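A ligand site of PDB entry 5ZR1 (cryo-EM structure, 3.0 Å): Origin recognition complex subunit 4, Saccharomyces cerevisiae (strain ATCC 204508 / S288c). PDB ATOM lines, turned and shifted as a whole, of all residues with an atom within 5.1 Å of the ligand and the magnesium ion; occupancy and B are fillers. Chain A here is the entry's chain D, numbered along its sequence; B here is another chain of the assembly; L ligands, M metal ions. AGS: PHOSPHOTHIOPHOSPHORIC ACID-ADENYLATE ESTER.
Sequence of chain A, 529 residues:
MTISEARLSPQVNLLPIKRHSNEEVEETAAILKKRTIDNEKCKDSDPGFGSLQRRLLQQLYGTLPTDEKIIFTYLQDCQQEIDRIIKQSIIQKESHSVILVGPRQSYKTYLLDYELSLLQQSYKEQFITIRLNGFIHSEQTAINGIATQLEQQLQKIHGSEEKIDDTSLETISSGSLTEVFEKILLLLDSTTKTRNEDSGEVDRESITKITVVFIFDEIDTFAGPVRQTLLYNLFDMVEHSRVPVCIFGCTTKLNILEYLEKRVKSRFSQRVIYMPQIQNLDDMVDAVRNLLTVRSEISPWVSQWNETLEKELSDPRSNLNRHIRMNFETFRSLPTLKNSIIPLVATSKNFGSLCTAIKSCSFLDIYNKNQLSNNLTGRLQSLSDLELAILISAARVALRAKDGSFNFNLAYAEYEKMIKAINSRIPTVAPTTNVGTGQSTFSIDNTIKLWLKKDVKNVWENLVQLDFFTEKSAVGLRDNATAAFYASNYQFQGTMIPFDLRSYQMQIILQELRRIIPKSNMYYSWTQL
The magnesium ion is bound by the side-chain hydroxyl (OG1) of Thr 109 and an oxygen (O2G) of the ligand.
The magnesium ion has two donor atoms within binding distance.
The backbone NH of Ser 106 is in hydrogen-bond range of an oxygen (O3A) of the ligand (3.4 Å).
The side-chain amide oxygen (OE1) of Gln 105 lies close to an oxygen (O2A) of the ligand, at 3.4 Å.
NZ of Lys 108 is in salt-bridge range of O1B of the ligand (2.7 Å).
O3B of the ligand is in hydrogen-bond range of N of Gln 105, 3.0 Å away.
N of Tyr 107 sits at hydrogen-bond distance from O3A of the ligand, at 3.2 Å.
The side-chain carboxylate (OD2) of Asp 113 is in hydrogen-bond range of a nitrogen (N6) of the ligand, at 3.1 Å.
The side-chain amino group of Lys 151 of chain B sits at hydrogen-bond distance from an oxygen (O3G) of the ligand, 3.4 Å away.
A sulfur (S1G) of the ligand lies close to the guanidinium group (NE) of Arg 104.
The backbone NH (N) of Thr 109 lies within hydrogen-bond range of an oxygen (O1A) of the ligand (3.1 Å).
The backbone NH (N) of Lys 108 lies within hydrogen-bond range of an oxygen (O1B) of the ligand.
The backbone NH (N) of Tyr 110 is in hydrogen-bond range of an oxygen (O1A) of the ligand, at 2.7 Å.
The backbone carbonyl oxygen (O) of Tyr 61 lies close to a nitrogen (N3) of the ligand.
Gly 62 touches the ligand.
NZ of Lys 69 touches N1 of the ligand, 3.7 Å away.
O of Pro 103 touches O1B of the ligand (3.999 Å).
Lys 338 touches the ligand.
Hydrophobic or aromatic side chains that line the ligand: Tyr 107 and Tyr 110.
Within 4 Å of the ligand: Tyr 61, Gly 62, Lys 69, Pro 103, Arg 104, Gln 105, Ser 106, Tyr 107, Lys 108, Thr 109, Tyr 110, Asp 113, Lys 338 and Lys 151 of chain B.
The nearest printed residue that does not touch the ligand is His 182 of chain B (4.1 Å).
Merely in contact with the magnesium ion: Glu 154 of chain B (3.2 Å).
NZ of Lys 151 of chain B sits close to ND1 of His 182 of chain B, 3.4 Å away.
A ring nitrogen (NE2) of His 182 of chain B sits close to the guanidinium group (NH1) of Arg 104 (3.3 Å).
The backbone carbonyl oxygen (O) of Pro 103 sits at hydrogen-bond distance from the side-chain amino group (NZ) of Lys 108, 3.4 Å away.
NH2 of Arg 104 is in salt-bridge range of OE2 of Glu 218, at 2.6 Å.
The side-chain amide nitrogen (NE2) of Gln 105 sits close to the backbone carbonyl oxygen (O) of His 182 of chain B, 3.3 Å away.
OH of Tyr 107 is in hydrogen-bond range of NZ of Lys 338, 2.9 Å away.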
ATOM      1  N   TYR A  61       2.094 -28.158  38.539  1.00  0.00           N
ATOM      2  CA  TYR A  61       1.510 -27.412  37.435  1.00  0.00           C
ATOM      3  C   TYR A  61       2.526 -27.054  36.367  1.00  0.00           C
ATOM      4  O   TYR A  61       2.133 -26.645  35.275  1.00  0.00           O
ATOM      5  CB  TYR A  61       0.832 -26.127  37.942  1.00  0.00           C
ATOM      6  CG  TYR A  61      -0.473 -26.366  38.662  1.00  0.00           C
ATOM      7  CD1 TYR A  61      -1.646 -26.600  37.960  1.00  0.00           C
ATOM      8  CD2 TYR A  61      -0.516 -26.368  40.042  1.00  0.00           C
ATOM      9  CE1 TYR A  61      -2.832 -26.816  38.629  1.00  0.00           C
ATOM     10  CE2 TYR A  61      -1.701 -26.594  40.707  1.00  0.00           C
ATOM     11  CZ  TYR A  61      -2.845 -26.812  40.005  1.00  0.00           C
ATOM     12  OH  TYR A  61      -4.020 -27.038  40.672  1.00  0.00           O
ATOM     13  N   GLY A  62       3.820 -27.207  36.649  1.00  0.00           N
ATOM     14  CA  GLY A  62       4.833 -26.876  35.678  1.00  0.00           C
ATOM     15  C   GLY A  62       5.168 -25.405  35.600  1.00  0.00           C
ATOM     16  O   GLY A  62       5.782 -24.986  34.611  1.00  0.00           O
ATOM     17  N   THR A  63       4.800 -24.610  36.592  1.00  0.00           N
ATOM     18  CA  THR A  63       5.074 -23.189  36.595  1.00  0.00           C
ATOM     19  C   THR A  63       6.370 -22.827  37.309  1.00  0.00           C
ATOM     20  O   THR A  63       6.490 -21.721  37.838  1.00  0.00           O
ATOM     21  CB  THR A  63       3.894 -22.429  37.217  1.00  0.00           C
ATOM     22  OG1 THR A  63       3.685 -22.897  38.554  1.00  0.00           O
ATOM     23  CG2 THR A  63       2.645 -22.653  36.412  1.00  0.00           C
ATOM     24  N   LYS A  69      12.542 -26.402  35.024  1.00  0.00           N
ATOM     25  CA  LYS A  69      11.370 -27.154  34.584  1.00  0.00           C
ATOM     26  C   LYS A  69      11.691 -28.622  34.359  1.00  0.00           C
ATOM     27  O   LYS A  69      12.767 -28.976  33.851  1.00  0.00           O
ATOM     28  CB  LYS A  69      10.771 -26.561  33.310  1.00  0.00           C
ATOM     29  CG  LYS A  69       9.888 -25.357  33.540  1.00  0.00           C
ATOM     30  CD  LYS A  69       9.110 -25.031  32.289  1.00  0.00           C
ATOM     31  CE  LYS A  69       8.138 -23.894  32.525  1.00  0.00           C
ATOM     32  NZ  LYS A  69       7.328 -23.617  31.304  1.00  0.00           N
ATOM     33  N   PRO A 103      -1.333 -38.064  21.407  1.00  0.00           N
ATOM     34  CA  PRO A 103      -2.680 -37.923  21.990  1.00  0.00           C
ATOM     35  C   PRO A 103      -2.896 -36.595  22.704  1.00  0.00           C
ATOM     36  O   PRO A 103      -2.001 -35.740  22.726  1.00  0.00           O
ATOM     37  CB  PRO A 103      -2.757 -39.109  22.962  1.00  0.00           C
ATOM     38  CG  PRO A 103      -1.346 -39.433  23.279  1.00  0.00           C
ATOM     39  CD  PRO A 103      -0.562 -39.147  22.043  1.00  0.00           C
ATOM     40  N   ARG A 104      -4.087 -36.393  23.234  1.00  0.00           N
ATOM     41  CA  ARG A 104      -4.336 -35.258  24.105  1.00  0.00           C
ATOM     42  C   ARG A 104      -3.553 -35.423  25.389  1.00  0.00           C
ATOM     43  O   ARG A 104      -3.375 -36.545  25.878  1.00  0.00           O
ATOM     44  CB  ARG A 104      -5.828 -35.140  24.390  1.00  0.00           C
ATOM     45  CG  ARG A 104      -6.637 -34.771  23.184  1.00  0.00           C
ATOM     46  CD  ARG A 104      -6.630 -33.287  22.992  1.00  0.00           C
ATOM     47  NE  ARG A 104      -7.003 -32.888  21.649  1.00  0.00           N
ATOM     48  CZ  ARG A 104      -8.253 -32.747  21.216  1.00  0.00           C
ATOM     49  NH1 ARG A 104      -9.265 -33.005  22.021  1.00  0.00           N
ATOM     50  NH2 ARG A 104      -8.468 -32.367  19.973  1.00  0.00           N
ATOM     51  N   GLN A 105      -3.046 -34.299  25.911  1.00  0.00           N
ATOM     52  CA  GLN A 105      -2.227 -34.230  27.129  1.00  0.00           C
ATOM     53  C   GLN A 105      -0.966 -35.082  27.001  1.00  0.00           C
ATOM     54  O   GLN A 105      -0.585 -35.820  27.907  1.00  0.00           O
ATOM     55  CB  GLN A 105      -3.044 -34.626  28.360  1.00  0.00           C
ATOM     56  CG  GLN A 105      -4.246 -33.751  28.560  1.00  0.00           C
ATOM     57  CD  GLN A 105      -3.876 -32.338  28.929  1.00  0.00           C
ATOM     58  OE1 GLN A 105      -3.936 -31.428  28.100  1.00  0.00           O
ATOM     59  NE2 GLN A 105      -3.570 -32.123  30.192  1.00  0.00           N
ATOM     60  N   SER A 106      -0.309 -34.942  25.853  1.00  0.00           N
ATOM     61  CA  SER A 106       0.930 -35.642  25.544  1.00  0.00           C
ATOM     62  C   SER A 106       2.124 -34.713  25.440  1.00  0.00           C
ATOM     63  O   SER A 106       3.094 -35.031  24.748  1.00  0.00           O
ATOM     64  CB  SER A 106       0.776 -36.441  24.254  1.00  0.00           C
ATOM     65  OG  SER A 106       1.996 -37.064  23.907  1.00  0.00           O
ATOM     66  N   TYR A 107       2.041 -33.534  26.079  1.00  0.00           N
ATOM     67  CA  TYR A 107       3.134 -32.568  26.215  1.00  0.00           C
ATOM     68  C   TYR A 107       3.583 -32.000  24.863  1.00  0.00           C
ATOM     69  O   TYR A 107       4.764 -31.724  24.661  1.00  0.00           O
ATOM     70  CB  TYR A 107       4.321 -33.152  26.974  1.00  0.00           C
ATOM     71  CG  TYR A 107       4.013 -33.567  28.394  1.00  0.00           C
ATOM     72  CD1 TYR A 107       3.918 -32.627  29.404  1.00  0.00           C
ATOM     73  CD2 TYR A 107       3.824 -34.899  28.720  1.00  0.00           C
ATOM     74  CE1 TYR A 107       3.627 -32.991  30.695  1.00  0.00           C
ATOM     75  CE2 TYR A 107       3.546 -35.281  30.006  1.00  0.00           C
ATOM     76  CZ  TYR A 107       3.452 -34.320  30.991  1.00  0.00           C
ATOM     77  OH  TYR A 107       3.163 -34.694  32.279  1.00  0.00           O
ATOM     78  N   LYS A 108       2.642 -31.817  23.934  1.00  0.00           N
ATOM     79  CA  LYS A 108       2.999 -31.157  22.682  1.00  0.00           C
ATOM     80  C   LYS A 108       3.168 -29.659  22.874  1.00  0.00           C
ATOM     81  O   LYS A 108       4.187 -29.095  22.483  1.00  0.00           O
ATOM     82  CB  LYS A 108       1.946 -31.443  21.618  1.00  0.00           C
ATOM     83  CG  LYS A 108       1.951 -32.859  21.123  1.00  0.00           C
ATOM     84  CD  LYS A 108       0.997 -33.057  19.977  1.00  0.00           C
ATOM     85  CE  LYS A 108      -0.262 -33.760  20.400  1.00  0.00           C
ATOM     86  NZ  LYS A 108      -1.166 -32.876  21.152  1.00  0.00           N
ATOM     87  N   THR A 109       2.164 -29.012  23.454  1.00  0.00           N
ATOM     88  CA  THR A 109       2.249 -27.588  23.757  1.00  0.00           C
ATOM     89  C   THR A 109       3.210 -27.335  24.905  1.00  0.00           C
ATOM     90  O   THR A 109       3.819 -26.254  24.979  1.00  0.00           O
ATOM     91  CB  THR A 109       0.848 -27.062  24.074  1.00  0.00           C
ATOM     92  OG1 THR A 109      -0.050 -27.494  23.049  1.00  0.00           O
ATOM     93  CG2 THR A 109       0.818 -25.549  24.106  1.00  0.00           C
ATOM     94  N   TYR A 110       3.396 -28.305  25.791  1.00  0.00           N
ATOM     95  CA  TYR A 110       4.341 -28.165  26.891  1.00  0.00           C
ATOM     96  C   TYR A 110       5.774 -28.100  26.390  1.00  0.00           C
ATOM     97  O   TYR A 110       6.563 -27.262  26.847  1.00  0.00           O
ATOM     98  CB  TYR A 110       4.190 -29.322  27.876  1.00  0.00           C
ATOM     99  CG  TYR A 110       5.151 -29.279  29.038  1.00  0.00           C
ATOM    100  CD1 TYR A 110       4.941 -28.416  30.099  1.00  0.00           C
ATOM    101  CD2 TYR A 110       6.283 -30.089  29.071  1.00  0.00           C
ATOM    102  CE1 TYR A 110       5.806 -28.369  31.163  1.00  0.00           C
ATOM    103  CE2 TYR A 110       7.159 -30.038  30.127  1.00  0.00           C
ATOM    104  CZ  TYR A 110       6.911 -29.183  31.170  1.00  0.00           C
ATOM    105  OH  TYR A 110       7.788 -29.132  32.226  1.00  0.00           O
ATOM    106  N   ASP A 113       6.286 -24.757  24.356  1.00  0.00           N
ATOM    107  CA  ASP A 113       6.437 -23.630  25.266  1.00  0.00           C
ATOM    108  C   ASP A 113       7.729 -23.729  26.058  1.00  0.00           C
ATOM    109  O   ASP A 113       8.254 -22.702  26.500  1.00  0.00           O
ATOM    110  CB  ASP A 113       5.257 -23.548  26.227  1.00  0.00           C
ATOM    111  CG  ASP A 113       3.986 -23.091  25.548  1.00  0.00           C
ATOM    112  OD1 ASP A 113       4.079 -22.381  24.530  1.00  0.00           O
ATOM    113  OD2 ASP A 113       2.896 -23.433  26.039  1.00  0.00           O
ATOM    114  N   ASP A 217      -2.024 -25.453  16.750  1.00  0.00           N
ATOM    115  CA  ASP A 217      -2.713 -26.452  17.543  1.00  0.00           C
ATOM    116  C   ASP A 217      -3.953 -26.864  16.752  1.00  0.00           C
ATOM    117  O   ASP A 217      -4.723 -26.002  16.331  1.00  0.00           O
ATOM    118  CB  ASP A 217      -3.095 -25.874  18.903  1.00  0.00           C
ATOM    119  CG  ASP A 217      -1.889 -25.414  19.698  1.00  0.00           C
ATOM    120  OD1 ASP A 217      -0.787 -25.962  19.485  1.00  0.00           O
ATOM    121  OD2 ASP A 217      -2.046 -24.486  20.521  1.00  0.00           O
ATOM    122  N   GLU A 218      -4.112 -28.174  16.548  1.00  0.00           N
ATOM    123  CA  GLU A 218      -5.121 -28.752  15.646  1.00  0.00           C
ATOM    124  C   GLU A 218      -4.984 -28.205  14.222  1.00  0.00           C
ATOM    125  O   GLU A 218      -5.830 -27.487  13.702  1.00  0.00           O
ATOM    126  CB  GLU A 218      -6.544 -28.596  16.192  1.00  0.00           C
ATOM    127  CG  GLU A 218      -7.002 -29.793  17.013  1.00  0.00           C
ATOM    128  CD  GLU A 218      -6.437 -29.844  18.410  1.00  0.00           C
ATOM    129  OE1 GLU A 218      -5.831 -28.844  18.864  1.00  0.00           O
ATOM    130  OE2 GLU A 218      -6.582 -30.904  19.055  1.00  0.00           O
ATOM    131  N   THR A 252      -3.606 -34.574  16.498  1.00  0.00           N
ATOM    132  CA  THR A 252      -3.804 -35.812  17.228  1.00  0.00           C
ATOM    133  C   THR A 252      -3.918 -37.015  16.304  1.00  0.00           C
ATOM    134  O   THR A 252      -3.565 -38.124  16.702  1.00  0.00           O
ATOM    135  CB  THR A 252      -5.081 -35.704  18.089  1.00  0.00           C
ATOM    136  OG1 THR A 252      -5.066 -34.457  18.780  1.00  0.00           O
ATOM    137  CG2 THR A 252      -5.120 -36.771  19.157  1.00  0.00           C
ATOM    138  N   PRO A 335      -0.801 -36.758  33.369  1.00  0.00           N
ATOM    139  CA  PRO A 335      -1.710 -35.682  33.816  1.00  0.00           C
ATOM    140  C   PRO A 335      -2.961 -36.135  34.546  1.00  0.00           C
ATOM    141  O   PRO A 335      -3.551 -35.315  35.259  1.00  0.00           O
ATOM    142  CB  PRO A 335      -2.059 -34.963  32.517  1.00  0.00           C
ATOM    143  CG  PRO A 335      -0.882 -35.097  31.719  1.00  0.00           C
ATOM    144  CD  PRO A 335      -0.369 -36.468  31.980  1.00  0.00           C
ATOM    145  N   LYS A 338      -1.691 -36.559  37.946  1.00  0.00           N
ATOM    146  CA  LYS A 338      -1.287 -35.236  38.393  1.00  0.00           C
ATOM    147  C   LYS A 338      -2.447 -34.475  39.018  1.00  0.00           C
ATOM    148  O   LYS A 338      -2.241 -33.757  40.001  1.00  0.00           O
ATOM    149  CB  LYS A 338      -0.694 -34.478  37.211  1.00  0.00           C
ATOM    150  CG  LYS A 338       0.074 -33.233  37.500  1.00  0.00           C
ATOM    151  CD  LYS A 338       0.537 -32.656  36.186  1.00  0.00           C
ATOM    152  CE  LYS A 338       1.656 -33.475  35.586  1.00  0.00           C
ATOM    153  NZ  LYS A 338       2.170 -32.868  34.323  1.00  0.00           N
ATOM    154  N   LYS B 151      -8.967 -23.817  25.339  1.00  0.00           N
ATOM    155  CA  LYS B 151      -7.713 -23.389  24.730  1.00  0.00           C
ATOM    156  C   LYS B 151      -7.553 -21.873  24.647  1.00  0.00           C
ATOM    157  O   LYS B 151      -6.658 -21.414  23.927  1.00  0.00           O
ATOM    158  CB  LYS B 151      -7.589 -23.987  23.339  1.00  0.00           C
ATOM    159  CG  LYS B 151      -7.578 -25.498  23.296  1.00  0.00           C
ATOM    160  CD  LYS B 151      -6.376 -26.062  24.010  1.00  0.00           C
ATOM    161  CE  LYS B 151      -6.237 -27.528  23.719  1.00  0.00           C
ATOM    162  NZ  LYS B 151      -7.353 -28.304  24.295  1.00  0.00           N
ATOM    163  N   GLU B 154      -4.026 -20.437  26.089  1.00  0.00           N
ATOM    164  CA  GLU B 154      -2.792 -20.539  25.311  1.00  0.00           C
ATOM    165  C   GLU B 154      -2.661 -19.433  24.282  1.00  0.00           C
ATOM    166  O   GLU B 154      -1.560 -19.210  23.767  1.00  0.00           O
ATOM    167  CB  GLU B 154      -2.748 -21.893  24.608  1.00  0.00           C
ATOM    168  CG  GLU B 154      -2.723 -23.061  25.568  1.00  0.00           C
ATOM    169  CD  GLU B 154      -2.812 -24.399  24.865  1.00  0.00           C
ATOM    170  OE1 GLU B 154      -2.993 -24.403  23.626  1.00  0.00           O
ATOM    171  OE2 GLU B 154      -2.702 -25.433  25.554  1.00  0.00           O
ATOM    172  N   HIS B 182      -8.878 -34.390  27.894  1.00  0.00           N
ATOM    173  CA  HIS B 182      -8.223 -33.129  28.187  1.00  0.00           C
ATOM    174  C   HIS B 182      -7.633 -33.081  29.583  1.00  0.00           C
ATOM    175  O   HIS B 182      -6.839 -32.180  29.849  1.00  0.00           O
ATOM    176  CB  HIS B 182      -9.193 -31.968  28.020  1.00  0.00           C
ATOM    177  CG  HIS B 182      -9.597 -31.708  26.608  1.00  0.00           C
ATOM    178  ND1 HIS B 182      -8.740 -31.136  25.690  1.00  0.00           N
ATOM    179  CD2 HIS B 182     -10.760 -31.914  25.951  1.00  0.00           C
ATOM    180  CE1 HIS B 182      -9.357 -31.018  24.529  1.00  0.00           C
ATOM    181  NE2 HIS B 182     -10.586 -31.478  24.662  1.00  0.00           N
HETATM  182  PG  AGS L   1      -3.503 -30.843  23.665  1.00  0.00           P
HETATM  183  S1G AGS L   1      -3.522 -31.794  21.965  1.00  0.00           S
HETATM  184  O2G AGS L   1      -2.925 -29.428  23.413  1.00  0.00           O
HETATM  185  O3G AGS L   1      -4.955 -30.699  24.203  1.00  0.00           O
HETATM  186  PB  AGS L   1      -1.071 -31.321  24.716  1.00  0.00           P
HETATM  187  O1B AGS L   1      -0.453 -32.186  23.707  1.00  0.00           O
HETATM  188  O2B AGS L   1      -0.912 -29.823  24.452  1.00  0.00           O
HETATM  189  O3B AGS L   1      -2.627 -31.576  24.714  1.00  0.00           O
HETATM  190  PA  AGS L   1       0.034 -30.343  26.981  1.00  0.00           P
HETATM  191  O1A AGS L   1       1.022 -29.567  26.248  1.00  0.00           O
HETATM  192  O2A AGS L   1      -1.216 -29.538  27.320  1.00  0.00           O
HETATM  193  O3A AGS L   1      -0.467 -31.574  26.147  1.00  0.00           O
HETATM  194  O5' AGS L   1       0.757 -30.950  28.244  1.00  0.00           O
HETATM  195  C5' AGS L   1       0.074 -31.673  29.277  1.00  0.00           C
HETATM  196  C4' AGS L   1       0.382 -31.071  30.628  1.00  0.00           C
HETATM  197  O4' AGS L   1       1.289 -29.954  30.474  1.00  0.00           O
HETATM  198  C3' AGS L   1      -0.826 -30.555  31.400  1.00  0.00           C
HETATM  199  O3' AGS L   1      -0.744 -30.902  32.768  1.00  0.00           O
HETATM  200  C2' AGS L   1      -0.739 -29.036  31.200  1.00  0.00           C
HETATM  201  O2' AGS L   1      -1.318 -28.333  32.280  1.00  0.00           O
HETATM  202  C1' AGS L   1       0.766 -28.833  31.153  1.00  0.00           C
HETATM  203  N9  AGS L   1       1.187 -27.628  30.439  1.00  0.00           N
HETATM  204  C8  AGS L   1       0.742 -27.197  29.218  1.00  0.00           C
HETATM  205  N7  AGS L   1       1.302 -26.081  28.812  1.00  0.00           N
HETATM  206  C5  AGS L   1       2.165 -25.754  29.846  1.00  0.00           C
HETATM  207  C6  AGS L   1       3.061 -24.680  30.031  1.00  0.00           C
HETATM  208  N6  AGS L   1       3.227 -23.692  29.154  1.00  0.00           N
HETATM  209  N1  AGS L   1       3.784 -24.659  31.174  1.00  0.00           N
HETATM  210  C2  AGS L   1       3.616 -25.642  32.063  1.00  0.00           C
HETATM  211  N3  AGS L   1       2.812 -26.704  31.992  1.00  0.00           N
HETATM  212  C4  AGS L   1       2.108 -26.702  30.850  1.00  0.00           C
HETATM  213 MG    MG M   1      -2.100 -27.537  23.207  1.00  0.00          MG
